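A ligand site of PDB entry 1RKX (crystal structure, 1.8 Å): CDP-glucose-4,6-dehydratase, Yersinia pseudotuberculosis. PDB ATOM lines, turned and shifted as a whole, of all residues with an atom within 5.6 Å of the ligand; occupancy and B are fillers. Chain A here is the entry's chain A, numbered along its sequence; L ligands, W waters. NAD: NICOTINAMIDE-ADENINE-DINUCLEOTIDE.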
ATOM      1  N   GLY A  16     -23.437  28.529  22.984  1.00  0.00           N
ATOM      2  CA  GLY A  16     -22.608  28.199  24.136  1.00  0.00           C
ATOM      3  C   GLY A  16     -22.843  29.110  25.324  1.00  0.00           C
ATOM      4  O   GLY A  16     -21.967  29.252  26.184  1.00  0.00           O
ATOM      5  N   HIS A  17     -24.006  29.751  25.374  1.00  0.00           N
ATOM      6  CA  HIS A  17     -24.335  30.649  26.483  1.00  0.00           C
ATOM      7  C   HIS A  17     -24.490  29.929  27.830  1.00  0.00           C
ATOM      8  O   HIS A  17     -24.473  30.576  28.878  1.00  0.00           O
ATOM      9  CB  HIS A  17     -25.620  31.425  26.176  1.00  0.00           C
ATOM     10  CG  HIS A  17     -26.864  30.605  26.260  1.00  0.00           C
ATOM     11  ND1 HIS A  17     -27.104  29.512  25.451  1.00  0.00           N
ATOM     12  CD2 HIS A  17     -27.968  30.727  27.048  1.00  0.00           C
ATOM     13  CE1 HIS A  17     -28.295  29.005  25.726  1.00  0.00           C
ATOM     14  NE2 HIS A  17     -28.836  29.730  26.691  1.00  0.00           N
ATOM     15  N   THR A  18     -24.657  28.611  27.812  1.00  0.00           N
ATOM     16  CA  THR A  18     -24.818  27.862  29.059  1.00  0.00           C
ATOM     17  C   THR A  18     -23.489  27.427  29.670  1.00  0.00           C
ATOM     18  O   THR A  18     -23.457  26.761  30.713  1.00  0.00           O
ATOM     19  CB  THR A  18     -25.666  26.584  28.861  1.00  0.00           C
ATOM     20  OG1 THR A  18     -25.023  25.717  27.935  1.00  0.00           O
ATOM     21  CG2 THR A  18     -27.063  26.946  28.338  1.00  0.00           C
ATOM     22  N   GLY A  19     -22.395  27.821  29.018  1.00  0.00           N
ATOM     23  CA  GLY A  19     -21.071  27.458  29.501  1.00  0.00           C
ATOM     24  C   GLY A  19     -20.390  28.554  30.317  1.00  0.00           C
ATOM     25  O   GLY A  19     -20.986  29.587  30.622  1.00  0.00           O
ATOM     26  N   PHE A  20     -19.129  28.309  30.651  1.00  0.00           N
ATOM     27  CA  PHE A  20     -18.345  29.253  31.448  1.00  0.00           C
ATOM     28  C   PHE A  20     -18.140  30.609  30.756  1.00  0.00           C
ATOM     29  O   PHE A  20     -18.590  31.644  31.264  1.00  0.00           O
ATOM     30  CB  PHE A  20     -16.990  28.621  31.794  1.00  0.00           C
ATOM     31  CG  PHE A  20     -16.034  29.534  32.514  1.00  0.00           C
ATOM     32  CD1 PHE A  20     -16.406  30.160  33.707  1.00  0.00           C
ATOM     33  CD2 PHE A  20     -14.746  29.747  32.024  1.00  0.00           C
ATOM     34  CE1 PHE A  20     -15.505  30.978  34.391  1.00  0.00           C
ATOM     35  CE2 PHE A  20     -13.839  30.552  32.701  1.00  0.00           C
ATOM     36  CZ  PHE A  20     -14.211  31.177  33.893  1.00  0.00           C
ATOM     37  N   LYS A  21     -17.453  30.606  29.619  1.00  0.00           N
ATOM     38  CA  LYS A  21     -17.205  31.862  28.899  1.00  0.00           C
ATOM     39  C   LYS A  21     -18.497  32.461  28.366  1.00  0.00           C
ATOM     40  O   LYS A  21     -18.690  33.679  28.421  1.00  0.00           O
ATOM     41  CB  LYS A  21     -16.216  31.635  27.743  1.00  0.00           C
ATOM     42  CG  LYS A  21     -14.801  31.263  28.194  1.00  0.00           C
ATOM     43  CD  LYS A  21     -13.873  31.011  27.012  1.00  0.00           C
ATOM     44  CE  LYS A  21     -13.689  32.271  26.171  1.00  0.00           C
ATOM     45  NZ  LYS A  21     -12.791  32.047  25.017  1.00  0.00           N
ATOM     46  N   GLY A  22     -19.366  31.602  27.856  1.00  0.00           N
ATOM     47  CA  GLY A  22     -20.639  32.059  27.311  1.00  0.00           C
ATOM     48  C   GLY A  22     -21.521  32.737  28.338  1.00  0.00           C
ATOM     49  O   GLY A  22     -22.212  33.708  28.037  1.00  0.00           O
ATOM     50  N   TYR A  39     -28.059  29.723  22.408  1.00  0.00           N
ATOM     51  CA  TYR A  39     -28.360  28.404  21.832  1.00  0.00           C
ATOM     52  C   TYR A  39     -27.230  27.483  22.294  1.00  0.00           C
ATOM     53  O   TYR A  39     -26.088  27.642  21.848  1.00  0.00           O
ATOM     54  CB  TYR A  39     -28.375  28.491  20.306  1.00  0.00           C
ATOM     55  CG  TYR A  39     -28.761  27.212  19.601  1.00  0.00           C
ATOM     56  CD1 TYR A  39     -30.076  27.005  19.165  1.00  0.00           C
ATOM     57  CD2 TYR A  39     -27.817  26.220  19.320  1.00  0.00           C
ATOM     58  CE1 TYR A  39     -30.443  25.844  18.484  1.00  0.00           C
ATOM     59  CE2 TYR A  39     -28.173  25.054  18.620  1.00  0.00           C
ATOM     60  CZ  TYR A  39     -29.481  24.879  18.209  1.00  0.00           C
ATOM     61  OH  TYR A  39     -29.843  23.741  17.518  1.00  0.00           O
ATOM     62  N   SER A  40     -27.555  26.538  23.176  1.00  0.00           N
ATOM     63  CA  SER A  40     -26.571  25.597  23.714  1.00  0.00           C
ATOM     64  C   SER A  40     -27.262  24.319  24.176  1.00  0.00           C
ATOM     65  O   SER A  40     -28.495  24.213  24.192  1.00  0.00           O
ATOM     66  CB  SER A  40     -25.869  26.167  24.963  1.00  0.00           C
ATOM     67  OG  SER A  40     -25.396  27.497  24.815  1.00  0.00           O
ATOM     68  N   LEU A  41     -26.447  23.351  24.576  1.00  0.00           N
ATOM     69  CA  LEU A  41     -26.979  22.130  25.149  1.00  0.00           C
ATOM     70  C   LEU A  41     -27.148  22.537  26.622  1.00  0.00           C
ATOM     71  O   LEU A  41     -26.692  23.605  27.021  1.00  0.00           O
ATOM     72  CB  LEU A  41     -25.976  20.987  25.073  1.00  0.00           C
ATOM     73  CG  LEU A  41     -25.602  20.430  23.699  1.00  0.00           C
ATOM     74  CD1 LEU A  41     -24.545  19.347  23.872  1.00  0.00           C
ATOM     75  CD2 LEU A  41     -26.831  19.867  23.004  1.00  0.00           C
ATOM     76  N   THR A  42     -27.781  21.695  27.423  1.00  0.00           N
ATOM     77  CA  THR A  42     -27.942  21.992  28.841  1.00  0.00           C
ATOM     78  C   THR A  42     -26.563  22.263  29.462  1.00  0.00           C
ATOM     79  O   THR A  42     -25.573  21.683  29.024  1.00  0.00           O
ATOM     80  CB  THR A  42     -28.590  20.793  29.572  1.00  0.00           C
ATOM     81  OG1 THR A  42     -29.943  20.638  29.107  1.00  0.00           O
ATOM     82  CG2 THR A  42     -28.599  21.007  31.075  1.00  0.00           C
ATOM     83  N   ALA A  43     -26.506  23.161  30.437  1.00  0.00           N
ATOM     84  CA  ALA A  43     -25.239  23.512  31.096  1.00  0.00           C
ATOM     85  C   ALA A  43     -24.411  22.244  31.306  1.00  0.00           C
ATOM     86  O   ALA A  43     -24.917  21.239  31.805  1.00  0.00           O
ATOM     87  CB  ALA A  43     -25.509  24.187  32.440  1.00  0.00           C
ATOM     88  N   PRO A  44     -23.118  22.292  30.943  1.00  0.00           N
ATOM     89  CA  PRO A  44     -22.179  21.168  31.054  1.00  0.00           C
ATOM     90  C   PRO A  44     -21.839  20.652  32.446  1.00  0.00           C
ATOM     91  O   PRO A  44     -21.386  19.510  32.587  1.00  0.00           O
ATOM     92  CB  PRO A  44     -20.947  21.689  30.334  1.00  0.00           C
ATOM     93  CG  PRO A  44     -20.952  23.140  30.708  1.00  0.00           C
ATOM     94  CD  PRO A  44     -22.408  23.506  30.486  1.00  0.00           C
ATOM     95  N   GLY A  64     -30.431  23.525  22.373  1.00  0.00           N
ATOM     96  CA  GLY A  64     -30.352  22.810  21.113  1.00  0.00           C
ATOM     97  C   GLY A  64     -28.928  22.404  20.788  1.00  0.00           C
ATOM     98  O   GLY A  64     -27.974  22.930  21.361  1.00  0.00           O
ATOM     99  N   ASP A  65     -28.784  21.466  19.862  1.00  0.00           N
ATOM    100  CA  ASP A  65     -27.472  20.976  19.466  1.00  0.00           C
ATOM    101  C   ASP A  65     -27.025  21.715  18.198  1.00  0.00           C
ATOM    102  O   ASP A  65     -27.794  21.830  17.253  1.00  0.00           O
ATOM    103  CB  ASP A  65     -27.564  19.474  19.178  1.00  0.00           C
ATOM    104  CG  ASP A  65     -26.216  18.793  19.190  1.00  0.00           C
ATOM    105  OD1 ASP A  65     -25.295  19.268  18.506  1.00  0.00           O
ATOM    106  OD2 ASP A  65     -26.089  17.763  19.892  1.00  0.00           O
ATOM    107  N   ILE A  66     -25.803  22.233  18.176  1.00  0.00           N
ATOM    108  CA  ILE A  66     -25.337  22.958  16.993  1.00  0.00           C
ATOM    109  C   ILE A  66     -25.114  22.011  15.821  1.00  0.00           C
ATOM    110  O   ILE A  66     -24.854  22.449  14.701  1.00  0.00           O
ATOM    111  CB  ILE A  66     -24.028  23.746  17.232  1.00  0.00           C
ATOM    112  CG1 ILE A  66     -22.920  22.805  17.683  1.00  0.00           C
ATOM    113  CG2 ILE A  66     -24.271  24.852  18.260  1.00  0.00           C
ATOM    114  CD1 ILE A  66     -21.569  23.491  17.830  1.00  0.00           C
ATOM    115  N   ARG A  67     -25.194  20.707  16.075  1.00  0.00           N
ATOM    116  CA  ARG A  67     -25.032  19.720  15.016  1.00  0.00           C
ATOM    117  C   ARG A  67     -26.377  19.481  14.313  1.00  0.00           C
ATOM    118  O   ARG A  67     -26.447  18.717  13.354  1.00  0.00           O
ATOM    119  CB  ARG A  67     -24.496  18.405  15.591  1.00  0.00           C
ATOM    120  CG  ARG A  67     -23.023  18.475  15.963  1.00  0.00           C
ATOM    121  CD  ARG A  67     -22.592  17.258  16.741  1.00  0.00           C
ATOM    122  NE  ARG A  67     -23.276  17.181  18.017  1.00  0.00           N
ATOM    123  CZ  ARG A  67     -22.990  16.298  18.971  1.00  0.00           C
ATOM    124  NH1 ARG A  67     -22.021  15.419  18.782  1.00  0.00           N
ATOM    125  NH2 ARG A  67     -23.671  16.308  20.113  1.00  0.00           N
ATOM    126  N   HIS A  86     -19.979  32.830  18.374  1.00  0.00           N
ATOM    127  CA  HIS A  86     -20.035  31.379  18.360  1.00  0.00           C
ATOM    128  C   HIS A  86     -19.047  30.811  19.370  1.00  0.00           C
ATOM    129  O   HIS A  86     -17.841  30.763  19.119  1.00  0.00           O
ATOM    130  CB  HIS A  86     -19.733  30.863  16.949  1.00  0.00           C
ATOM    131  CG  HIS A  86     -19.705  29.365  16.848  1.00  0.00           C
ATOM    132  ND1 HIS A  86     -20.691  28.557  17.358  1.00  0.00           N
ATOM    133  CD2 HIS A  86     -18.795  28.529  16.267  1.00  0.00           C
ATOM    134  CE1 HIS A  86     -20.407  27.286  17.099  1.00  0.00           C
ATOM    135  NE2 HIS A  86     -19.259  27.246  16.441  1.00  0.00           N
ATOM    136  N   MET A  87     -19.571  30.374  20.520  1.00  0.00           N
ATOM    137  CA  MET A  87     -18.721  29.796  21.554  1.00  0.00           C
ATOM    138  C   MET A  87     -19.009  28.348  21.869  1.00  0.00           C
ATOM    139  O   MET A  87     -18.272  27.714  22.631  1.00  0.00           O
ATOM    140  CB  MET A  87     -18.810  30.638  22.835  1.00  0.00           C
ATOM    141  CG  MET A  87     -18.110  31.979  22.708  1.00  0.00           C
ATOM    142  SD  MET A  87     -17.675  32.708  24.294  1.00  0.00           S
ATOM    143  CE  MET A  87     -19.195  33.498  24.683  1.00  0.00           C
ATOM    144  N   ALA A  88     -20.063  27.798  21.287  1.00  0.00           N
ATOM    145  CA  ALA A  88     -20.407  26.400  21.523  1.00  0.00           C
ATOM    146  C   ALA A  88     -19.383  25.478  20.873  1.00  0.00           C
ATOM    147  O   ALA A  88     -19.031  25.647  19.703  1.00  0.00           O
ATOM    148  CB  ALA A  88     -21.798  26.097  20.965  1.00  0.00           C
ATOM    149  N   ALA A  89     -18.907  24.507  21.646  1.00  0.00           N
ATOM    150  CA  ALA A  89     -17.925  23.542  21.148  1.00  0.00           C
ATOM    151  C   ALA A  89     -17.651  22.482  22.207  1.00  0.00           C
ATOM    152  O   ALA A  89     -18.008  22.654  23.378  1.00  0.00           O
ATOM    153  CB  ALA A  89     -16.615  24.255  20.801  1.00  0.00           C
ATOM    154  N   GLN A  90     -17.023  21.392  21.784  1.00  0.00           N
ATOM    155  CA  GLN A  90     -16.592  20.308  22.687  1.00  0.00           C
ATOM    156  C   GLN A  90     -15.210  20.890  22.992  1.00  0.00           C
ATOM    157  O   GLN A  90     -14.293  20.785  22.170  1.00  0.00           O
ATOM    158  CB  GLN A  90     -16.480  18.992  21.917  1.00  0.00           C
ATOM    159  CG  GLN A  90     -16.256  17.749  22.776  1.00  0.00           C
ATOM    160  CD  GLN A  90     -15.042  17.860  23.662  1.00  0.00           C
ATOM    161  OE1 GLN A  90     -15.102  18.445  24.742  1.00  0.00           O
ATOM    162  NE2 GLN A  90     -13.921  17.319  23.210  1.00  0.00           N
ATOM    163  N   PRO A  91     -15.042  21.508  24.170  1.00  0.00           N
ATOM    164  CA  PRO A  91     -13.787  22.145  24.589  1.00  0.00           C
ATOM    165  C   PRO A  91     -12.708  21.344  25.302  1.00  0.00           C
ATOM    166  O   PRO A  91     -11.658  21.890  25.617  1.00  0.00           O
ATOM    167  CB  PRO A  91     -14.293  23.264  25.479  1.00  0.00           C
ATOM    168  CG  PRO A  91     -15.336  22.531  26.278  1.00  0.00           C
ATOM    169  CD  PRO A  91     -16.067  21.673  25.221  1.00  0.00           C
ATOM    170  N   THR A 106     -18.988  18.423  16.270  1.00  0.00           N
ATOM    171  CA  THR A 106     -19.382  19.617  17.016  1.00  0.00           C
ATOM    172  C   THR A 106     -18.570  20.862  16.663  1.00  0.00           C
ATOM    173  O   THR A 106     -19.139  21.919  16.369  1.00  0.00           O
ATOM    174  CB  THR A 106     -19.256  19.384  18.546  1.00  0.00           C
ATOM    175  OG1 THR A 106     -20.097  18.288  18.929  1.00  0.00           O
ATOM    176  CG2 THR A 106     -19.683  20.628  19.315  1.00  0.00           C
ATOM    177  N   ILE A 130     -15.314  31.943  18.142  1.00  0.00           N
ATOM    178  CA  ILE A 130     -14.328  31.560  19.136  1.00  0.00           C
ATOM    179  C   ILE A 130     -13.757  30.191  18.781  1.00  0.00           C
ATOM    180  O   ILE A 130     -14.476  29.187  18.753  1.00  0.00           O
ATOM    181  CB  ILE A 130     -14.938  31.478  20.563  1.00  0.00           C
ATOM    182  CG1 ILE A 130     -15.181  32.884  21.118  1.00  0.00           C
ATOM    183  CG2 ILE A 130     -14.001  30.711  21.494  1.00  0.00           C
ATOM    184  CD1 ILE A 130     -16.195  33.692  20.359  1.00  0.00           C
ATOM    185  N   THR A 131     -12.469  30.150  18.488  1.00  0.00           N
ATOM    186  CA  THR A 131     -11.829  28.896  18.169  1.00  0.00           C
ATOM    187  C   THR A 131     -11.004  28.491  19.391  1.00  0.00           C
ATOM    188  O   THR A 131     -11.581  28.017  20.387  1.00  0.00           O
ATOM    189  CB  THR A 131     -10.955  29.022  16.884  1.00  0.00           C
ATOM    190  OG1 THR A 131      -9.963  30.040  17.063  1.00  0.00           O
ATOM    191  CG2 THR A 131     -11.840  29.377  15.699  1.00  0.00           C
ATOM    192  N   SER A 132      -9.691  28.687  19.362  1.00  0.00           N
ATOM    193  CA  SER A 132      -8.871  28.329  20.519  1.00  0.00           C
ATOM    194  C   SER A 132      -7.425  28.771  20.326  1.00  0.00           C
ATOM    195  O   SER A 132      -6.996  28.997  19.199  1.00  0.00           O
ATOM    196  CB  SER A 132      -8.897  26.813  20.724  1.00  0.00           C
ATOM    197  OG  SER A 132      -8.023  26.403  21.773  1.00  0.00           O
ATOM    198  N   ASP A 133      -6.687  28.895  21.424  1.00  0.00           N
ATOM    199  CA  ASP A 133      -5.278  29.248  21.310  1.00  0.00           C
ATOM    200  C   ASP A 133      -4.557  28.014  20.747  1.00  0.00           C
ATOM    201  O   ASP A 133      -3.463  28.103  20.213  1.00  0.00           O
ATOM    202  CB  ASP A 133      -4.709  29.645  22.693  1.00  0.00           C
ATOM    203  CG  ASP A 133      -4.781  28.524  23.714  1.00  0.00           C
ATOM    204  OD1 ASP A 133      -5.837  27.866  23.822  1.00  0.00           O
ATOM    205  OD2 ASP A 133      -3.783  28.315  24.435  1.00  0.00           O
ATOM    206  N   TYR A 157      -9.240  17.694  19.612  1.00  0.00           N
ATOM    207  CA  TYR A 157      -9.807  18.983  20.002  1.00  0.00           C
ATOM    208  C   TYR A 157      -9.024  20.129  19.337  1.00  0.00           C
ATOM    209  O   TYR A 157      -9.601  20.965  18.628  1.00  0.00           O
ATOM    210  CB  TYR A 157      -9.770  19.172  21.529  1.00  0.00           C
ATOM    211  CG  TYR A 157      -9.844  20.623  21.944  1.00  0.00           C
ATOM    212  CD1 TYR A 157     -11.044  21.337  21.875  1.00  0.00           C
ATOM    213  CD2 TYR A 157      -8.695  21.308  22.347  1.00  0.00           C
ATOM    214  CE1 TYR A 157     -11.101  22.701  22.201  1.00  0.00           C
ATOM    215  CE2 TYR A 157      -8.737  22.672  22.660  1.00  0.00           C
ATOM    216  CZ  TYR A 157      -9.938  23.358  22.589  1.00  0.00           C
ATOM    217  OH  TYR A 157      -9.966  24.694  22.887  1.00  0.00           O
ATOM    218  N   LYS A 161     -10.144  22.656  16.109  1.00  0.00           N
ATOM    219  CA  LYS A 161     -10.168  24.113  16.183  1.00  0.00           C
ATOM    220  C   LYS A 161      -9.364  24.688  15.023  1.00  0.00           C
ATOM    221  O   LYS A 161      -9.689  25.758  14.476  1.00  0.00           O
ATOM    222  CB  LYS A 161      -9.608  24.584  17.525  1.00  0.00           C
ATOM    223  CG  LYS A 161     -10.554  24.325  18.708  1.00  0.00           C
ATOM    224  CD  LYS A 161     -11.840  25.167  18.586  1.00  0.00           C
ATOM    225  CE  LYS A 161     -12.704  25.078  19.837  1.00  0.00           C
ATOM    226  NZ  LYS A 161     -13.815  26.083  19.815  1.00  0.00           N
ATOM    227  N   ALA A 193      -7.861  32.393  22.034  1.00  0.00           N
ATOM    228  CA  ALA A 193      -7.450  32.633  23.414  1.00  0.00           C
ATOM    229  C   ALA A 193      -7.538  31.357  24.228  1.00  0.00           C
ATOM    230  O   ALA A 193      -8.260  30.431  23.875  1.00  0.00           O
ATOM    231  CB  ALA A 193      -8.343  33.715  24.034  1.00  0.00           C
ATOM    232  N   GLY A 194      -6.787  31.289  25.324  1.00  0.00           N
ATOM    233  CA  GLY A 194      -6.831  30.095  26.146  1.00  0.00           C
ATOM    234  C   GLY A 194      -6.511  30.392  27.590  1.00  0.00           C
ATOM    235  O   GLY A 194      -6.351  31.551  27.981  1.00  0.00           O
ATOM    236  N   ASN A 195      -6.412  29.335  28.397  1.00  0.00           N
ATOM    237  CA  ASN A 195      -6.083  29.462  29.817  1.00  0.00           C
ATOM    238  C   ASN A 195      -6.965  30.458  30.541  1.00  0.00           C
ATOM    239  O   ASN A 195      -6.484  31.289  31.305  1.00  0.00           O
ATOM    240  CB  ASN A 195      -4.620  29.875  29.952  1.00  0.00           C
ATOM    241  CG  ASN A 195      -3.721  29.166  28.945  1.00  0.00           C
ATOM    242  OD1 ASN A 195      -3.527  27.962  29.012  1.00  0.00           O
ATOM    243  ND2 ASN A 195      -3.190  29.929  28.008  1.00  0.00           N
ATOM    244  N   VAL A 196      -8.270  30.372  30.304  1.00  0.00           N
ATOM    245  CA  VAL A 196      -9.207  31.293  30.917  1.00  0.00           C
ATOM    246  C   VAL A 196      -9.628  30.807  32.310  1.00  0.00           C
ATOM    247  O   VAL A 196      -9.997  29.648  32.490  1.00  0.00           O
ATOM    248  CB  VAL A 196     -10.457  31.460  30.024  1.00  0.00           C
ATOM    249  CG1 VAL A 196     -11.418  32.430  30.655  1.00  0.00           C
ATOM    250  CG2 VAL A 196     -10.045  31.965  28.651  1.00  0.00           C
ATOM    251  N   ASP A 201     -16.337  28.598  37.044  1.00  0.00           N
ATOM    252  CA  ASP A 201     -15.954  27.528  36.134  1.00  0.00           C
ATOM    253  C   ASP A 201     -15.821  26.257  36.946  1.00  0.00           C
ATOM    254  O   ASP A 201     -14.946  26.143  37.800  1.00  0.00           O
ATOM    255  CB  ASP A 201     -14.643  27.825  35.426  1.00  0.00           C
ATOM    256  CG  ASP A 201     -14.252  26.717  34.448  1.00  0.00           C
ATOM    257  OD1 ASP A 201     -15.157  25.976  33.990  1.00  0.00           O
ATOM    258  OD2 ASP A 201     -13.054  26.588  34.140  1.00  0.00           O
HETATM  259  PA  NAD L   1     -17.864  25.197  28.538  1.00  0.00           P
HETATM  260  O1A NAD L   1     -17.865  23.727  28.465  1.00  0.00           O
HETATM  261  O2A NAD L   1     -18.106  25.816  29.852  1.00  0.00           O
HETATM  262  O5B NAD L   1     -18.956  25.807  27.499  1.00  0.00           O
HETATM  263  C5B NAD L   1     -19.197  25.110  26.264  1.00  0.00           C
HETATM  264  C4B NAD L   1     -20.580  25.458  25.727  1.00  0.00           C
HETATM  265  O4B NAD L   1     -20.657  24.667  24.529  1.00  0.00           O
HETATM  266  C3B NAD L   1     -21.703  24.963  26.637  1.00  0.00           C
HETATM  267  O3B NAD L   1     -22.610  26.058  26.840  1.00  0.00           O
HETATM  268  C2B NAD L   1     -22.277  23.790  25.852  1.00  0.00           C
HETATM  269  O2B NAD L   1     -23.671  23.513  26.092  1.00  0.00           O
HETATM  270  C1B NAD L   1     -21.956  24.174  24.431  1.00  0.00           C
HETATM  271  N9A NAD L   1     -21.963  23.042  23.540  1.00  0.00           N
HETATM  272  C8A NAD L   1     -21.062  22.001  23.486  1.00  0.00           C
HETATM  273  N7A NAD L   1     -21.363  21.102  22.562  1.00  0.00           N
HETATM  274  C5A NAD L   1     -22.520  21.578  21.984  1.00  0.00           C
HETATM  275  C6A NAD L   1     -23.324  21.070  20.941  1.00  0.00           C
HETATM  276  N6A NAD L   1     -23.113  19.955  20.275  1.00  0.00           N
HETATM  277  N1A NAD L   1     -24.435  21.784  20.590  1.00  0.00           N
HETATM  278  C2A NAD L   1     -24.690  22.955  21.281  1.00  0.00           C
HETATM  279  N3A NAD L   1     -24.009  23.522  22.259  1.00  0.00           N
HETATM  280  C4A NAD L   1     -22.915  22.775  22.573  1.00  0.00           C
HETATM  281  O3  NAD L   1     -16.525  25.697  27.958  1.00  0.00           O
HETATM  282  PN  NAD L   1     -15.913  27.204  27.839  1.00  0.00           P
HETATM  283  O1N NAD L   1     -14.733  27.183  28.713  1.00  0.00           O
HETATM  284  O2N NAD L   1     -16.958  28.176  28.279  1.00  0.00           O
HETATM  285  O5D NAD L   1     -15.463  27.277  26.333  1.00  0.00           O
HETATM  286  C5D NAD L   1     -16.086  28.279  25.512  1.00  0.00           C
HETATM  287  C4D NAD L   1     -15.472  28.252  24.135  1.00  0.00           C
HETATM  288  O4D NAD L   1     -14.102  28.708  24.317  1.00  0.00           O
HETATM  289  C3D NAD L   1     -15.335  26.909  23.426  1.00  0.00           C
HETATM  290  O3D NAD L   1     -15.418  27.119  22.007  1.00  0.00           O
HETATM  291  C2D NAD L   1     -13.935  26.470  23.827  1.00  0.00           C
HETATM  292  O2D NAD L   1     -13.420  25.511  22.889  1.00  0.00           O
HETATM  293  C1D NAD L   1     -13.203  27.776  23.782  1.00  0.00           C
HETATM  294  N1N NAD L   1     -11.964  27.724  24.556  1.00  0.00           N
HETATM  295  C2N NAD L   1     -11.946  27.845  25.951  1.00  0.00           C
HETATM  296  C3N NAD L   1     -10.656  27.876  26.709  1.00  0.00           C
HETATM  297  C7N NAD L   1     -10.737  28.069  28.159  1.00  0.00           C
HETATM  298  O7N NAD L   1      -9.664  28.118  28.786  1.00  0.00           O
HETATM  299  N7N NAD L   1     -11.910  28.201  28.820  1.00  0.00           N
HETATM  300  C4N NAD L   1      -9.365  27.631  25.954  1.00  0.00           C
HETATM  301  C5N NAD L   1      -9.568  27.488  24.480  1.00  0.00           C
HETATM  302  C6N NAD L   1     -10.731  27.534  23.856  1.00  0.00           C
HETATM  303  O   HOH W   1     -16.882  27.681  19.667  1.00  0.00           O
HETATM  304  O   HOH W   2     -19.975  18.891  23.289  1.00  0.00           O
HETATM  305  O   HOH W   3     -21.219  17.909  21.305  1.00  0.00           O
HETATM  306  O   HOH W   4     -13.310  24.584  28.951  1.00  0.00           O
HETATM  307  O   HOH W   5     -11.451  24.577  24.966  1.00  0.00           O
HETATM  308  O   HOH W   6     -14.270  25.650  31.157  1.00  0.00           O
HETATM  309  O   HOH W   7      -7.064  26.753  28.050  1.00  0.00           O
HETATM  310  O   HOH W   8     -23.157  21.367  27.768  1.00  0.00           O
HETATM  311  O   HOH W   9     -19.158  29.068  26.994  1.00  0.00           O
HETATM  312  O   HOH W  10     -11.123  30.502  23.632  1.00  0.00           O
HETATM  313  O   HOH W  11     -19.278  20.142  25.823  1.00  0.00           O
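Water W9 lies within hydrogen-bond range of N of Gly 22, O2N of the ligand, O of Gly 16 and N of Lys 21.
Water W8 lies within hydrogen-bond range of the backbone carbonyl oxygen (O) of Thr 42 (2.7 Å) and an oxygen (O2B) of the ligand (2.8 Å).
Water W6 bridges an oxygen (O1N) of the ligand (2.9 Å) and the side-chain carboxylate (OD1) of Asp 201 (3.0 Å).
Water W3 lies within hydrogen-bond range of the side-chain hydroxyl of Thr 106 (2.7 Å), a nitrogen (N6A) of the ligand (3.0 Å) and the guanidinium group of Arg 67 (3.2 Å).
Water W10 bridges the side-chain amino group of Lys 21 (2.7 Å) and the backbone carbonyl oxygen of Ala 193 (2.9 Å).
Water W5 lies within hydrogen-bond range of OH of Tyr 157 (2.6 Å), O of Pro 91 (2.8 Å) and O2D of the ligand (3.0 Å).
The backbone NH of Ala 89 sits at hydrogen-bond distance from an oxygen (O4B) of the ligand.
An oxygen (O3B) of the ligand lies within hydrogen-bond range of the backbone NH (N) of Gly 19.
An oxygen (O2B) of the ligand is in hydrogen-bond range of the backbone carbonyl oxygen (O) of Leu 41 (3.2 Å).
The backbone carbonyl oxygen of Met 87 sits at hydrogen-bond distance from an oxygen (O3D) of the ligand (3.0 Å).
The backbone NH (N) of Thr 18 lies close to an oxygen (O3B) of the ligand (3.4 Å).
An oxygen (O2B) of the ligand is in hydrogen-bond range of the backbone NH (N) of Leu 41 (3.2 Å).
The backbone NH (N) of Ile 66 lies within hydrogen-bond range of a nitrogen (N1A) of the ligand, 2.8 Å away.
A nitrogen (N6A) of the ligand lies within hydrogen-bond range of the side-chain carboxylate of Asp 65 (2.9 Å).
The backbone NH (N) of Val 196 lies within hydrogen-bond range of an oxygen (O7N) of the ligand (3.1 Å).
N of Lys 21 is in hydrogen-bond range of O2N of the ligand, 2.8 Å away.
O of Gly 16 lies within hydrogen-bond range of O3B of the ligand (3.3 Å).
The side-chain amino group (NZ) of Lys 161 is in hydrogen-bond range of an oxygen (O3D) of the ligand.
An oxygen (O2A) of the ligand lies within hydrogen-bond range of the backbone NH (N) of Phe 20 (2.8 Å).
An oxygen (O3B) of the ligand lies within hydrogen-bond range of the side-chain hydroxyl (OG1) of Thr 18, 2.7 Å away.
The backbone NH (N) of Asn 195 is in hydrogen-bond range of an oxygen (O7N) of the ligand (3.5 Å).
Merely in contact with the ligand: Tyr 157 (3.1 Å), Ala 193 (3.3 Å), Gly 64 (3.3 Å), Ser 132 (3.3 Å), Ile 130 (3.5 Å), Ala 88 (3.5 Å), Pro 91 (3.5 Å), Gly 194 (3.5 Å), Arg 67 (3.6 Å), Ser 40 (3.6 Å), Thr 131 (3.6 Å), Thr 106 (3.6 Å), Asp 133 (3.8 Å), Pro 44 (3.9 Å) and Thr 42 (3.9 Å).
Hydrophobic or aromatic side chains that line the ligand: Phe 20, Leu 41, Pro 44, Ile 66, Ala 88, Ala 89, Pro 91, Ile 130, Tyr 157 and Val 196.
28 residues have an atom within 4 Å of the ligand: Gly 16, Thr 18, Gly 19, Phe 20, Lys 21, Ser 40, Leu 41, Thr 42, Pro 44, Gly 64, Asp 65, Ile 66, Arg 67, Met 87, Ala 88, Ala 89, Pro 91, Thr 106, Ile 130, Thr 131, Ser 132, Asp 133, Tyr 157, Lys 161, Ala 193, Gly 194, Asn 195 and Val 196.
OG of Ser 40 sits at hydrogen-bond distance from N of His 17 (2.7 Å).
N of Ile 130 lies within hydrogen-bond range of O of His 86, 3.0 Å away.
OG of Ser 40 lies within hydrogen-bond range of N of Gly 16, at 2.9 Å.
O of Ile 130 is in hydrogen-bond range of NZ of Lys 161, at 3.3 Å.
The side-chain hydroxyl of Tyr 157 lies within hydrogen-bond range of the side-chain hydroxyl of Ser 132.
The side-chain hydroxyl (OH) of Tyr 39 sits at hydrogen-bond distance from the backbone carbonyl oxygen (O) of Asp 65 (2.8 Å).
The side-chain carboxylate of Asp 65 is in salt-bridge range of the guanidinium group of Arg 67, 2.8 Å away.
The guanidinium group (NH1) of Arg 67 sits at hydrogen-bond distance from the side-chain hydroxyl (OG1) of Thr 106.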
